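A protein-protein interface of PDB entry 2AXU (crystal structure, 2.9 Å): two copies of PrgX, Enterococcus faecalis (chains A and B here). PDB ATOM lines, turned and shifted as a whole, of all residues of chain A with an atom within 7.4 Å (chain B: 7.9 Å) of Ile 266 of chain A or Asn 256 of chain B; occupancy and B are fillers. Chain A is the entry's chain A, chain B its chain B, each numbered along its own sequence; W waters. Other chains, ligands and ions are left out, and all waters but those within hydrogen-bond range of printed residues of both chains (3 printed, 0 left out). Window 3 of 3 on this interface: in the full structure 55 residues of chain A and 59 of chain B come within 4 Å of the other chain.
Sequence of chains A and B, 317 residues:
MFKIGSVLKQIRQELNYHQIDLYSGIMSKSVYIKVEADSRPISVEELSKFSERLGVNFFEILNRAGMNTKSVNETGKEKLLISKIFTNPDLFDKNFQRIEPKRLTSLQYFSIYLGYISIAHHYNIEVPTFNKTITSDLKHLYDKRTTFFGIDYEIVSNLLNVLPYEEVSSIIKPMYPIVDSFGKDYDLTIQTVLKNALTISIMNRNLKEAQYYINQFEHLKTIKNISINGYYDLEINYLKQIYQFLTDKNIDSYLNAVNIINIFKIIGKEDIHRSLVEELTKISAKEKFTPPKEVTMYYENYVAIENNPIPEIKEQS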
ATOM      1  N   ASN A 259     -25.735  20.173  25.712  1.00  0.00           N
ATOM      2  CA  ASN A 259     -24.471  20.688  25.199  1.00  0.00           C
ATOM      3  C   ASN A 259     -23.406  20.799  26.296  1.00  0.00           C
ATOM      4  O   ASN A 259     -22.246  20.420  26.091  1.00  0.00           O
ATOM      5  CB  ASN A 259     -24.682  22.048  24.520  1.00  0.00           C
ATOM      6  CG  ASN A 259     -23.387  22.644  24.000  1.00  0.00           C
ATOM      7  OD1 ASN A 259     -22.517  21.924  23.508  1.00  0.00           O
ATOM      8  ND2 ASN A 259     -23.258  23.964  24.088  1.00  0.00           N
ATOM      9  N   ILE A 260     -23.785  21.312  27.463  1.00  0.00           N
ATOM     10  CA  ILE A 260     -22.820  21.431  28.537  1.00  0.00           C
ATOM     11  C   ILE A 260     -22.347  20.042  28.933  1.00  0.00           C
ATOM     12  O   ILE A 260     -21.161  19.834  29.195  1.00  0.00           O
ATOM     13  CB  ILE A 260     -23.414  22.174  29.756  1.00  0.00           C
ATOM     14  CG1 ILE A 260     -23.546  23.663  29.419  1.00  0.00           C
ATOM     15  CG2 ILE A 260     -22.520  21.976  30.985  1.00  0.00           C
ATOM     16  CD1 ILE A 260     -24.185  24.503  30.504  1.00  0.00           C
ATOM     17  N   ILE A 261     -23.271  19.089  28.960  1.00  0.00           N
ATOM     18  CA  ILE A 261     -22.929  17.716  29.311  1.00  0.00           C
ATOM     19  C   ILE A 261     -21.864  17.212  28.339  1.00  0.00           C
ATOM     20  O   ILE A 261     -21.000  16.410  28.702  1.00  0.00           O
ATOM     21  CB  ILE A 261     -24.179  16.785  29.254  1.00  0.00           C
ATOM     22  CG1 ILE A 261     -24.906  16.817  30.597  1.00  0.00           C
ATOM     23  CG2 ILE A 261     -23.777  15.357  28.909  1.00  0.00           C
ATOM     24  CD1 ILE A 261     -26.102  15.889  30.669  1.00  0.00           C
ATOM     25  N   ASN A 262     -21.915  17.704  27.107  1.00  0.00           N
ATOM     26  CA  ASN A 262     -20.955  17.280  26.100  1.00  0.00           C
ATOM     27  C   ASN A 262     -19.569  17.884  26.320  1.00  0.00           C
ATOM     28  O   ASN A 262     -18.562  17.212  26.102  1.00  0.00           O
ATOM     29  CB  ASN A 262     -21.451  17.632  24.701  1.00  0.00           C
ATOM     30  CG  ASN A 262     -20.544  17.089  23.619  1.00  0.00           C
ATOM     31  OD1 ASN A 262     -20.374  15.875  23.486  1.00  0.00           O
ATOM     32  ND2 ASN A 262     -19.949  17.984  22.841  1.00  0.00           N
ATOM     33  N   ILE A 263     -19.511  19.145  26.743  1.00  0.00           N
ATOM     34  CA  ILE A 263     -18.230  19.792  26.991  1.00  0.00           C
ATOM     35  C   ILE A 263     -17.449  18.979  28.017  1.00  0.00           C
ATOM     36  O   ILE A 263     -16.234  18.792  27.895  1.00  0.00           O
ATOM     37  CB  ILE A 263     -18.416  21.215  27.530  1.00  0.00           C
ATOM     38  CG1 ILE A 263     -19.000  22.109  26.440  1.00  0.00           C
ATOM     39  CG2 ILE A 263     -17.089  21.769  28.002  1.00  0.00           C
ATOM     40  CD1 ILE A 263     -18.128  22.228  25.208  1.00  0.00           C
ATOM     41  N   PHE A 264     -18.154  18.501  29.035  1.00  0.00           N
ATOM     42  CA  PHE A 264     -17.519  17.706  30.060  1.00  0.00           C
ATOM     43  C   PHE A 264     -16.894  16.470  29.436  1.00  0.00           C
ATOM     44  O   PHE A 264     -15.918  15.928  29.961  1.00  0.00           O
ATOM     45  CB  PHE A 264     -18.531  17.320  31.142  1.00  0.00           C
ATOM     46  CG  PHE A 264     -18.746  18.396  32.167  1.00  0.00           C
ATOM     47  CD1 PHE A 264     -17.692  18.809  32.973  1.00  0.00           C
ATOM     48  CD2 PHE A 264     -19.980  19.027  32.302  1.00  0.00           C
ATOM     49  CE1 PHE A 264     -17.850  19.831  33.894  1.00  0.00           C
ATOM     50  CE2 PHE A 264     -20.152  20.062  33.230  1.00  0.00           C
ATOM     51  CZ  PHE A 264     -19.083  20.465  34.026  1.00  0.00           C
ATOM     52  N   LYS A 265     -17.434  16.022  28.308  1.00  0.00           N
ATOM     53  CA  LYS A 265     -16.864  14.852  27.652  1.00  0.00           C
ATOM     54  C   LYS A 265     -15.671  15.272  26.797  1.00  0.00           C
ATOM     55  O   LYS A 265     -14.654  14.583  26.755  1.00  0.00           O
ATOM     56  CB  LYS A 265     -17.891  14.153  26.768  1.00  0.00           C
ATOM     57  CG  LYS A 265     -17.376  12.841  26.198  1.00  0.00           C
ATOM     58  CD  LYS A 265     -18.169  12.413  24.980  1.00  0.00           C
ATOM     59  CE  LYS A 265     -18.020  13.409  23.833  1.00  0.00           C
ATOM     60  NZ  LYS A 265     -18.708  12.959  22.594  1.00  0.00           N
ATOM     61  N   ILE A 266     -15.793  16.409  26.120  1.00  0.00           N
ATOM     62  CA  ILE A 266     -14.711  16.888  25.276  1.00  0.00           C
ATOM     63  C   ILE A 266     -13.463  17.229  26.081  1.00  0.00           C
ATOM     64  O   ILE A 266     -12.357  16.875  25.679  1.00  0.00           O
ATOM     65  CB  ILE A 266     -15.125  18.131  24.451  1.00  0.00           C
ATOM     66  CG1 ILE A 266     -16.161  17.740  23.398  1.00  0.00           C
ATOM     67  CG2 ILE A 266     -13.901  18.742  23.766  1.00  0.00           C
ATOM     68  CD1 ILE A 266     -16.588  18.885  22.491  1.00  0.00           C
ATOM     69  N   ILE A 267     -13.628  17.903  27.214  1.00  0.00           N
ATOM     70  CA  ILE A 267     -12.462  18.265  28.005  1.00  0.00           C
ATOM     71  C   ILE A 267     -11.921  17.118  28.848  1.00  0.00           C
ATOM     72  O   ILE A 267     -10.986  17.296  29.622  1.00  0.00           O
ATOM     73  CB  ILE A 267     -12.737  19.481  28.915  1.00  0.00           C
ATOM     74  CG1 ILE A 267     -13.633  19.083  30.090  1.00  0.00           C
ATOM     75  CG2 ILE A 267     -13.363  20.604  28.094  1.00  0.00           C
ATOM     76  CD1 ILE A 267     -13.719  20.144  31.171  1.00  0.00           C
ATOM     77  N   GLY A 268     -12.517  15.942  28.710  1.00  0.00           N
ATOM     78  CA  GLY A 268     -12.030  14.788  29.442  1.00  0.00           C
ATOM     79  C   GLY A 268     -12.493  14.517  30.863  1.00  0.00           C
ATOM     80  O   GLY A 268     -12.042  13.545  31.474  1.00  0.00           O
ATOM     81  N   LYS A 269     -13.371  15.352  31.408  1.00  0.00           N
ATOM     82  CA  LYS A 269     -13.860  15.130  32.768  1.00  0.00           C
ATOM     83  C   LYS A 269     -14.819  13.945  32.748  1.00  0.00           C
ATOM     84  O   LYS A 269     -16.033  14.113  32.715  1.00  0.00           O
ATOM     85  CB  LYS A 269     -14.568  16.384  33.280  1.00  0.00           C
ATOM     86  CG  LYS A 269     -13.658  17.608  33.380  1.00  0.00           C
ATOM     87  CD  LYS A 269     -12.591  17.423  34.457  1.00  0.00           C
ATOM     88  CE  LYS A 269     -13.204  17.443  35.848  1.00  0.00           C
ATOM     89  NZ  LYS A 269     -12.204  17.086  36.890  1.00  0.00           N
ATOM     90  N   HIS A 273     -19.014  13.578  33.611  1.00  0.00           N
ATOM     91  CA  HIS A 273     -19.817  13.298  32.433  1.00  0.00           C
ATOM     92  C   HIS A 273     -20.697  12.091  32.720  1.00  0.00           C
ATOM     93  O   HIS A 273     -21.834  12.017  32.262  1.00  0.00           O
ATOM     94  CB  HIS A 273     -18.921  13.028  31.219  1.00  0.00           C
ATOM     95  CG  HIS A 273     -19.677  12.642  29.987  1.00  0.00           C
ATOM     96  ND1 HIS A 273     -19.863  11.328  29.608  1.00  0.00           N
ATOM     97  CD2 HIS A 273     -20.330  13.395  29.069  1.00  0.00           C
ATOM     98  CE1 HIS A 273     -20.595  11.291  28.509  1.00  0.00           C
ATOM     99  NE2 HIS A 273     -20.892  12.533  28.161  1.00  0.00           N
ATOM    100  N   LYS B 221      -2.485  17.385  35.558  1.00  0.00           N
ATOM    101  CA  LYS B 221      -3.652  16.630  35.993  1.00  0.00           C
ATOM    102  C   LYS B 221      -3.311  15.339  36.725  1.00  0.00           C
ATOM    103  O   LYS B 221      -4.107  14.843  37.518  1.00  0.00           O
ATOM    104  CB  LYS B 221      -4.546  16.322  34.791  1.00  0.00           C
ATOM    105  CG  LYS B 221      -5.165  17.558  34.170  1.00  0.00           C
ATOM    106  CD  LYS B 221      -6.054  17.196  33.012  1.00  0.00           C
ATOM    107  CE  LYS B 221      -6.600  18.441  32.355  1.00  0.00           C
ATOM    108  NZ  LYS B 221      -7.477  18.114  31.195  1.00  0.00           N
ATOM    109  N   ASP B 233      -8.767  24.759  31.832  1.00  0.00           N
ATOM    110  CA  ASP B 233      -8.952  23.444  31.239  1.00  0.00           C
ATOM    111  C   ASP B 233      -9.830  23.534  29.999  1.00  0.00           C
ATOM    112  O   ASP B 233      -9.542  22.926  28.963  1.00  0.00           O
ATOM    113  CB  ASP B 233      -9.585  22.498  32.257  1.00  0.00           C
ATOM    114  CG  ASP B 233      -9.512  21.058  31.819  1.00  0.00           C
ATOM    115  OD1 ASP B 233      -8.936  20.814  30.738  1.00  0.00           O
ATOM    116  OD2 ASP B 233     -10.012  20.171  32.542  1.00  0.00           O
ATOM    117  N   LEU B 234     -10.904  24.304  30.115  1.00  0.00           N
ATOM    118  CA  LEU B 234     -11.836  24.491  29.018  1.00  0.00           C
ATOM    119  C   LEU B 234     -11.184  25.295  27.891  1.00  0.00           C
ATOM    120  O   LEU B 234     -11.341  24.964  26.712  1.00  0.00           O
ATOM    121  CB  LEU B 234     -13.096  25.192  29.539  1.00  0.00           C
ATOM    122  CG  LEU B 234     -14.335  25.312  28.654  1.00  0.00           C
ATOM    123  CD1 LEU B 234     -14.622  24.010  27.926  1.00  0.00           C
ATOM    124  CD2 LEU B 234     -15.506  25.691  29.541  1.00  0.00           C
ATOM    125  N   ASN B 237      -8.258  23.413  26.182  1.00  0.00           N
ATOM    126  CA  ASN B 237      -8.807  22.370  25.328  1.00  0.00           C
ATOM    127  C   ASN B 237      -9.299  23.031  24.047  1.00  0.00           C
ATOM    128  O   ASN B 237      -9.303  22.418  22.981  1.00  0.00           O
ATOM    129  CB  ASN B 237      -9.952  21.633  26.025  1.00  0.00           C
ATOM    130  CG  ASN B 237     -10.275  20.312  25.360  1.00  0.00           C
ATOM    131  OD1 ASN B 237     -10.968  20.264  24.343  1.00  0.00           O
ATOM    132  ND2 ASN B 237      -9.756  19.228  25.924  1.00  0.00           N
ATOM    133  N   TYR B 238      -9.716  24.287  24.152  1.00  0.00           N
ATOM    134  CA  TYR B 238     -10.157  25.027  22.976  1.00  0.00           C
ATOM    135  C   TYR B 238      -8.955  25.179  22.040  1.00  0.00           C
ATOM    136  O   TYR B 238      -9.057  24.974  20.827  1.00  0.00           O
ATOM    137  CB  TYR B 238     -10.679  26.410  23.370  1.00  0.00           C
ATOM    138  CG  TYR B 238     -10.541  27.433  22.267  1.00  0.00           C
ATOM    139  CD1 TYR B 238      -9.458  28.311  22.236  1.00  0.00           C
ATOM    140  CD2 TYR B 238     -11.464  27.486  21.224  1.00  0.00           C
ATOM    141  CE1 TYR B 238      -9.295  29.216  21.189  1.00  0.00           C
ATOM    142  CE2 TYR B 238     -11.313  28.383  20.173  1.00  0.00           C
ATOM    143  CZ  TYR B 238     -10.225  29.243  20.159  1.00  0.00           C
ATOM    144  OH  TYR B 238     -10.060  30.110  19.102  1.00  0.00           O
ATOM    145  N   LYS B 240      -6.422  23.291  22.007  1.00  0.00           N
ATOM    146  CA  LYS B 240      -6.074  21.952  21.544  1.00  0.00           C
ATOM    147  C   LYS B 240      -6.844  21.651  20.266  1.00  0.00           C
ATOM    148  O   LYS B 240      -6.311  21.040  19.342  1.00  0.00           O
ATOM    149  CB  LYS B 240      -6.418  20.898  22.599  1.00  0.00           C
ATOM    150  CG  LYS B 240      -5.774  19.549  22.326  1.00  0.00           C
ATOM    151  CD  LYS B 240      -6.336  18.444  23.208  1.00  0.00           C
ATOM    152  CE  LYS B 240      -7.652  17.891  22.666  1.00  0.00           C
ATOM    153  NZ  LYS B 240      -8.133  16.709  23.447  1.00  0.00           N
ATOM    154  N   GLN B 241      -8.104  22.079  20.222  1.00  0.00           N
ATOM    155  CA  GLN B 241      -8.942  21.861  19.047  1.00  0.00           C
ATOM    156  C   GLN B 241      -8.408  22.685  17.874  1.00  0.00           C
ATOM    157  O   GLN B 241      -8.330  22.193  16.745  1.00  0.00           O
ATOM    158  CB  GLN B 241     -10.400  22.257  19.331  1.00  0.00           C
ATOM    159  CG  GLN B 241     -11.095  21.500  20.474  1.00  0.00           C
ATOM    160  CD  GLN B 241     -11.297  20.018  20.196  1.00  0.00           C
ATOM    161  OE1 GLN B 241     -11.496  19.604  19.052  1.00  0.00           O
ATOM    162  NE2 GLN B 241     -11.266  19.213  21.253  1.00  0.00           N
ATOM    163  N   ILE B 242      -8.047  23.941  18.140  1.00  0.00           N
ATOM    164  CA  ILE B 242      -7.509  24.813  17.095  1.00  0.00           C
ATOM    165  C   ILE B 242      -6.227  24.177  16.584  1.00  0.00           C
ATOM    166  O   ILE B 242      -5.904  24.244  15.398  1.00  0.00           O
ATOM    167  CB  ILE B 242      -7.159  26.211  17.638  1.00  0.00           C
ATOM    168  CG1 ILE B 242      -8.421  26.922  18.134  1.00  0.00           C
ATOM    169  CG2 ILE B 242      -6.462  27.025  16.553  1.00  0.00           C
ATOM    170  CD1 ILE B 242      -9.310  27.454  17.028  1.00  0.00           C
ATOM    171  N   GLN B 244      -5.517  20.965  16.424  1.00  0.00           N
ATOM    172  CA  GLN B 244      -5.842  19.857  15.534  1.00  0.00           C
ATOM    173  C   GLN B 244      -6.302  20.399  14.188  1.00  0.00           C
ATOM    174  O   GLN B 244      -6.047  19.796  13.149  1.00  0.00           O
ATOM    175  CB  GLN B 244      -6.928  18.977  16.160  1.00  0.00           C
ATOM    176  CG  GLN B 244      -6.443  18.223  17.393  1.00  0.00           C
ATOM    177  CD  GLN B 244      -7.572  17.708  18.270  1.00  0.00           C
ATOM    178  OE1 GLN B 244      -7.334  17.170  19.354  1.00  0.00           O
ATOM    179  NE2 GLN B 244      -8.807  17.869  17.809  1.00  0.00           N
ATOM    180  N   ASN B 250      -8.982  19.673  10.427  1.00  0.00           N
ATOM    181  CA  ASN B 250     -10.014  18.767  10.897  1.00  0.00           C
ATOM    182  C   ASN B 250     -11.262  19.602  11.170  1.00  0.00           C
ATOM    183  O   ASN B 250     -11.276  20.429  12.084  1.00  0.00           O
ATOM    184  CB  ASN B 250      -9.548  18.086  12.179  1.00  0.00           C
ATOM    185  CG  ASN B 250     -10.529  17.059  12.683  1.00  0.00           C
ATOM    186  OD1 ASN B 250     -11.704  17.356  12.904  1.00  0.00           O
ATOM    187  ND2 ASN B 250     -10.050  15.837  12.878  1.00  0.00           N
ATOM    188  N   ILE B 251     -12.303  19.388  10.370  1.00  0.00           N
ATOM    189  CA  ILE B 251     -13.549  20.127  10.517  1.00  0.00           C
ATOM    190  C   ILE B 251     -14.215  19.910  11.878  1.00  0.00           C
ATOM    191  O   ILE B 251     -14.726  20.861  12.479  1.00  0.00           O
ATOM    192  CB  ILE B 251     -14.537  19.769   9.371  1.00  0.00           C
ATOM    193  CG1 ILE B 251     -14.132  20.515   8.096  1.00  0.00           C
ATOM    194  CG2 ILE B 251     -15.974  20.108   9.772  1.00  0.00           C
ATOM    195  CD1 ILE B 251     -14.106  22.031   8.255  1.00  0.00           C
ATOM    196  N   ASP B 252     -14.211  18.671  12.365  1.00  0.00           N
ATOM    197  CA  ASP B 252     -14.817  18.389  13.660  1.00  0.00           C
ATOM    198  C   ASP B 252     -14.139  19.221  14.724  1.00  0.00           C
ATOM    199  O   ASP B 252     -14.805  19.844  15.548  1.00  0.00           O
ATOM    200  CB  ASP B 252     -14.703  16.909  14.032  1.00  0.00           C
ATOM    201  CG  ASP B 252     -15.781  16.064  13.389  1.00  0.00           C
ATOM    202  OD1 ASP B 252     -16.904  16.579  13.197  1.00  0.00           O
ATOM    203  OD2 ASP B 252     -15.512  14.884  13.090  1.00  0.00           O
ATOM    204  N   SER B 253     -12.810  19.227  14.705  1.00  0.00           N
ATOM    205  CA  SER B 253     -12.023  19.993  15.666  1.00  0.00           C
ATOM    206  C   SER B 253     -12.426  21.458  15.641  1.00  0.00           C
ATOM    207  O   SER B 253     -12.590  22.080  16.693  1.00  0.00           O
ATOM    208  CB  SER B 253     -10.537  19.876  15.340  1.00  0.00           C
ATOM    209  OG  SER B 253     -10.093  18.544  15.503  1.00  0.00           O
ATOM    210  N   TYR B 254     -12.588  22.005  14.439  1.00  0.00           N
ATOM    211  CA  TYR B 254     -12.969  23.403  14.302  1.00  0.00           C
ATOM    212  C   TYR B 254     -14.301  23.683  14.984  1.00  0.00           C
ATOM    213  O   TYR B 254     -14.454  24.688  15.689  1.00  0.00           O
ATOM    214  CB  TYR B 254     -13.044  23.801  12.824  1.00  0.00           C
ATOM    215  CG  TYR B 254     -13.123  25.293  12.620  1.00  0.00           C
ATOM    216  CD1 TYR B 254     -14.335  25.974  12.735  1.00  0.00           C
ATOM    217  CD2 TYR B 254     -11.973  26.034  12.371  1.00  0.00           C
ATOM    218  CE1 TYR B 254     -14.397  27.361  12.612  1.00  0.00           C
ATOM    219  CE2 TYR B 254     -12.020  27.419  12.243  1.00  0.00           C
ATOM    220  CZ  TYR B 254     -13.233  28.075  12.367  1.00  0.00           C
ATOM    221  OH  TYR B 254     -13.276  29.445  12.255  1.00  0.00           O
ATOM    222  N   LEU B 255     -15.265  22.789  14.777  1.00  0.00           N
ATOM    223  CA  LEU B 255     -16.584  22.948  15.376  1.00  0.00           C
ATOM    224  C   LEU B 255     -16.546  22.835  16.898  1.00  0.00           C
ATOM    225  O   LEU B 255     -17.368  23.435  17.584  1.00  0.00           O
ATOM    226  CB  LEU B 255     -17.558  21.922  14.788  1.00  0.00           C
ATOM    227  CG  LEU B 255     -17.831  22.103  13.291  1.00  0.00           C
ATOM    228  CD1 LEU B 255     -18.717  20.981  12.776  1.00  0.00           C
ATOM    229  CD2 LEU B 255     -18.488  23.457  13.058  1.00  0.00           C
ATOM    230  N   ASN B 256     -15.598  22.069  17.428  1.00  0.00           N
ATOM    231  CA  ASN B 256     -15.479  21.926  18.875  1.00  0.00           C
ATOM    232  C   ASN B 256     -14.997  23.254  19.437  1.00  0.00           C
ATOM    233  O   ASN B 256     -15.416  23.681  20.518  1.00  0.00           O
ATOM    234  CB  ASN B 256     -14.478  20.832  19.238  1.00  0.00           C
ATOM    235  CG  ASN B 256     -14.948  19.458  18.825  1.00  0.00           C
ATOM    236  OD1 ASN B 256     -16.057  19.042  19.164  1.00  0.00           O
ATOM    237  ND2 ASN B 256     -14.103  18.735  18.096  1.00  0.00           N
ATOM    238  N   ALA B 257     -14.107  23.905  18.695  1.00  0.00           N
ATOM    239  CA  ALA B 257     -13.584  25.192  19.113  1.00  0.00           C
ATOM    240  C   ALA B 257     -14.754  26.150  19.234  1.00  0.00           C
ATOM    241  O   ALA B 257     -14.943  26.788  20.270  1.00  0.00           O
ATOM    242  CB  ALA B 257     -12.587  25.708  18.091  1.00  0.00           C
ATOM    243  N   VAL B 258     -15.544  26.238  18.169  1.00  0.00           N
ATOM    244  CA  VAL B 258     -16.701  27.123  18.163  1.00  0.00           C
ATOM    245  C   VAL B 258     -17.654  26.806  19.314  1.00  0.00           C
ATOM    246  O   VAL B 258     -18.142  27.708  19.995  1.00  0.00           O
ATOM    247  CB  VAL B 258     -17.473  27.022  16.839  1.00  0.00           C
ATOM    248  CG1 VAL B 258     -18.716  27.893  16.898  1.00  0.00           C
ATOM    249  CG2 VAL B 258     -16.583  27.451  15.685  1.00  0.00           C
ATOM    250  N   ASN B 259     -17.916  25.523  19.535  1.00  0.00           N
ATOM    251  CA  ASN B 259     -18.815  25.115  20.604  1.00  0.00           C
ATOM    252  C   ASN B 259     -18.295  25.568  21.964  1.00  0.00           C
ATOM    253  O   ASN B 259     -19.060  26.045  22.806  1.00  0.00           O
ATOM    254  CB  ASN B 259     -19.013  23.596  20.592  1.00  0.00           C
ATOM    255  CG  ASN B 259     -19.932  23.126  21.704  1.00  0.00           C
ATOM    256  OD1 ASN B 259     -20.965  23.741  21.965  1.00  0.00           O
ATOM    257  ND2 ASN B 259     -19.565  22.029  22.361  1.00  0.00           N
ATOM    258  N   ILE B 260     -16.993  25.422  22.182  1.00  0.00           N
ATOM    259  CA  ILE B 260     -16.409  25.835  23.449  1.00  0.00           C
ATOM    260  C   ILE B 260     -16.486  27.348  23.623  1.00  0.00           C
ATOM    261  O   ILE B 260     -16.667  27.844  24.734  1.00  0.00           O
ATOM    262  CB  ILE B 260     -14.948  25.367  23.568  1.00  0.00           C
ATOM    263  CG1 ILE B 260     -14.915  23.841  23.681  1.00  0.00           C
ATOM    264  CG2 ILE B 260     -14.291  26.016  24.779  1.00  0.00           C
ATOM    265  CD1 ILE B 260     -13.532  23.249  23.678  1.00  0.00           C
ATOM    266  N   ILE B 261     -16.348  28.078  22.522  1.00  0.00           N
ATOM    267  CA  ILE B 261     -16.444  29.532  22.571  1.00  0.00           C
ATOM    268  C   ILE B 261     -17.850  29.856  23.052  1.00  0.00           C
ATOM    269  O   ILE B 261     -18.061  30.762  23.862  1.00  0.00           O
ATOM    270  CB  ILE B 261     -16.256  30.174  21.178  1.00  0.00           C
ATOM    271  CG1 ILE B 261     -14.793  30.075  20.752  1.00  0.00           C
ATOM    272  CG2 ILE B 261     -16.722  31.619  21.210  1.00  0.00           C
ATOM    273  CD1 ILE B 261     -14.505  30.743  19.427  1.00  0.00           C
ATOM    274  N   ASN B 262     -18.811  29.091  22.548  1.00  0.00           N
ATOM    275  CA  ASN B 262     -20.203  29.289  22.906  1.00  0.00           C
ATOM    276  C   ASN B 262     -20.440  29.050  24.393  1.00  0.00           C
ATOM    277  O   ASN B 262     -21.076  29.865  25.066  1.00  0.00           O
ATOM    278  CB  ASN B 262     -21.098  28.365  22.083  1.00  0.00           C
ATOM    279  CG  ASN B 262     -22.564  28.695  22.241  1.00  0.00           C
ATOM    280  OD1 ASN B 262     -22.985  29.824  21.988  1.00  0.00           O
ATOM    281  ND2 ASN B 262     -23.350  27.712  22.663  1.00  0.00           N
ATOM    282  N   ILE B 263     -19.927  27.933  24.904  1.00  0.00           N
ATOM    283  CA  ILE B 263     -20.089  27.611  26.313  1.00  0.00           C
ATOM    284  C   ILE B 263     -19.638  28.770  27.189  1.00  0.00           C
ATOM    285  O   ILE B 263     -20.267  29.075  28.207  1.00  0.00           O
ATOM    286  CB  ILE B 263     -19.285  26.361  26.699  1.00  0.00           C
ATOM    287  CG1 ILE B 263     -19.967  25.121  26.128  1.00  0.00           C
ATOM    288  CG2 ILE B 263     -19.184  26.247  28.214  1.00  0.00           C
ATOM    289  CD1 ILE B 263     -21.368  24.883  26.678  1.00  0.00           C
HETATM  290  O   HOH W   1      -8.491  17.007  28.042  1.00  0.00           O
HETATM  291  O   HOH W   2      -9.958  17.732  31.921  1.00  0.00           O
HETATM  292  O   HOH W   3      -9.202  19.856  28.264  1.00  0.00           O
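Of chain B, only Asn 237 (3.4 Å), Gln 241 (3.7 Å) and Asn 256 (3.4 Å) come within 4 Å of Ile 266 of chain A.
Asn 256 of chain B touches just one residue of chain A: Ile 266.
Of the printed residues of chain B, Ile 267 of chain A touches Lys 221, Asp 233, Leu 234 and Asn 237.
Of the printed residues of chain A, Ile 263 of chain B touches Asn 259, Ile 260 and Ile 263.
Asn 250 of chain B touches none of the printed residues of chain A.
The nearest residue of chain B that does not touch Ile 266 of chain A is Asn 259 of chain B (4.3 Å).
The nearest printed residue of chain A that does not touch Lys 221 of chain B is Gly 268 of chain A (5.9 Å).
Asn 259 of chain A touches Ile 263 of chain B.
Ile 260 of chain A touches Ile 263 of chain B (CG1 to CD1, 3.7 Å).
Ile 263 of chain A touches Leu 234 of chain B (CG2 to CD1, 3.3 Å).
Asn 259 of chain B touches Ile 263 of chain A.
CG1 of Ile 263 of chain B touches CG1 of Ile 263 of chain A (3.2 Å).
Ile 266 of chain A touches Asn 237 of chain B (CG2 to OD1, 3.4 Å).
NE2 of Gln 241 of chain B touches CG2 of Ile 266 of chain A, at 3.7 Å.
Ile 266 of chain A touches Asn 256 of chain B (CD1 to OD1, 3.4 Å).
NZ of Lys 221 of chain B touches O of Ile 267 of chain A, at 3.9 Å.
Asp 233 of chain B touches Ile 267 of chain A (OD2 to CD1, 3.95 Å).
Asn 259 of chain B touches its own counterpart, Asn 259 of chain A.
Asn 259 of chain A touches Ile 263 of chain B, and with the chains exchanged Ile 263 of chain A touches Asn 259 of chain B.
Ile 260 of chain A touches Ile 263 of chain B, and with the chains exchanged Ile 263 of chain A touches Ile 260 of chain B.
Ile 263 of chain A touches its own counterpart, Ile 263 of chain B.
5 positions are printed for both chains.
Of the 14 pairs that touch across the chains among the printed residues, 6 have their exchanged pair printed and touching as well.
OD1 of Asn 237 of chain B is in hydrogen-bond range of NE2 of Gln 241 of chain B (3.3 Å).
OE1 of Gln 241 of chain B is in hydrogen-bond range of ND2 of Asn 256 of chain B (2.9 Å).
The side-chain amino group of Lys 221 of chain B lies within salt-bridge range of the side-chain carboxylate of Asp 233 of chain B (3.1 Å).
O of Asp 252 of chain B lies within hydrogen-bond range of ND2 of Asn 256 of chain B, 2.9 Å away.
The side-chain amide oxygen (OE1) of Gln 241 of chain B sits at hydrogen-bond distance from the side-chain amide nitrogen (NE2) of Gln 244 of chain B, at 3.4 Å.
Printed residues of chain A that touch a printed residue of chain B: Asn 259, Ile 260, Ile 263, Ile 266 and Ile 267.
Printed residues of chain B that touch a printed residue of chain A: Lys 221, Asp 233, Leu 234, Asn 237, Gln 241, Asn 256, Asn 259, Ile 260 and Ile 263.
Hydrophobic or aromatic side chains of chain B that line the printed part of chain A: Leu 234, Ile 260 and Ile 263.
Among the printed residues, no Asp or Glu carboxylate lies within 4 Å of a Lys or Arg side-chain nitrogen of the other chain.
OD1 of Asn 259 of chain B lies close to OD1 of Asn 259 of chain A, 2.8 Å away.
Water W3 lies within hydrogen-bond range of the side-chain amide nitrogen of Asn 237 of chain B, the side-chain carboxylate of Asp 233 of chain B and the backbone carbonyl oxygen of Ile 267 of chain A.
Water W2 lies within hydrogen-bond range of the side-chain carboxylate of Asp 233 of chain B (2.5 Å), the backbone carbonyl oxygen of Ile 267 of chain A (2.6 Å) and the side-chain amino group of Lys 221 of chain B (2.6 Å).
Water W1 lies within hydrogen-bond range of O of Ile 267 of chain A (3.0 Å), ND2 of Asn 237 of chain B (3.3 Å) and NZ of Lys 221 of chain B (3.5 Å).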
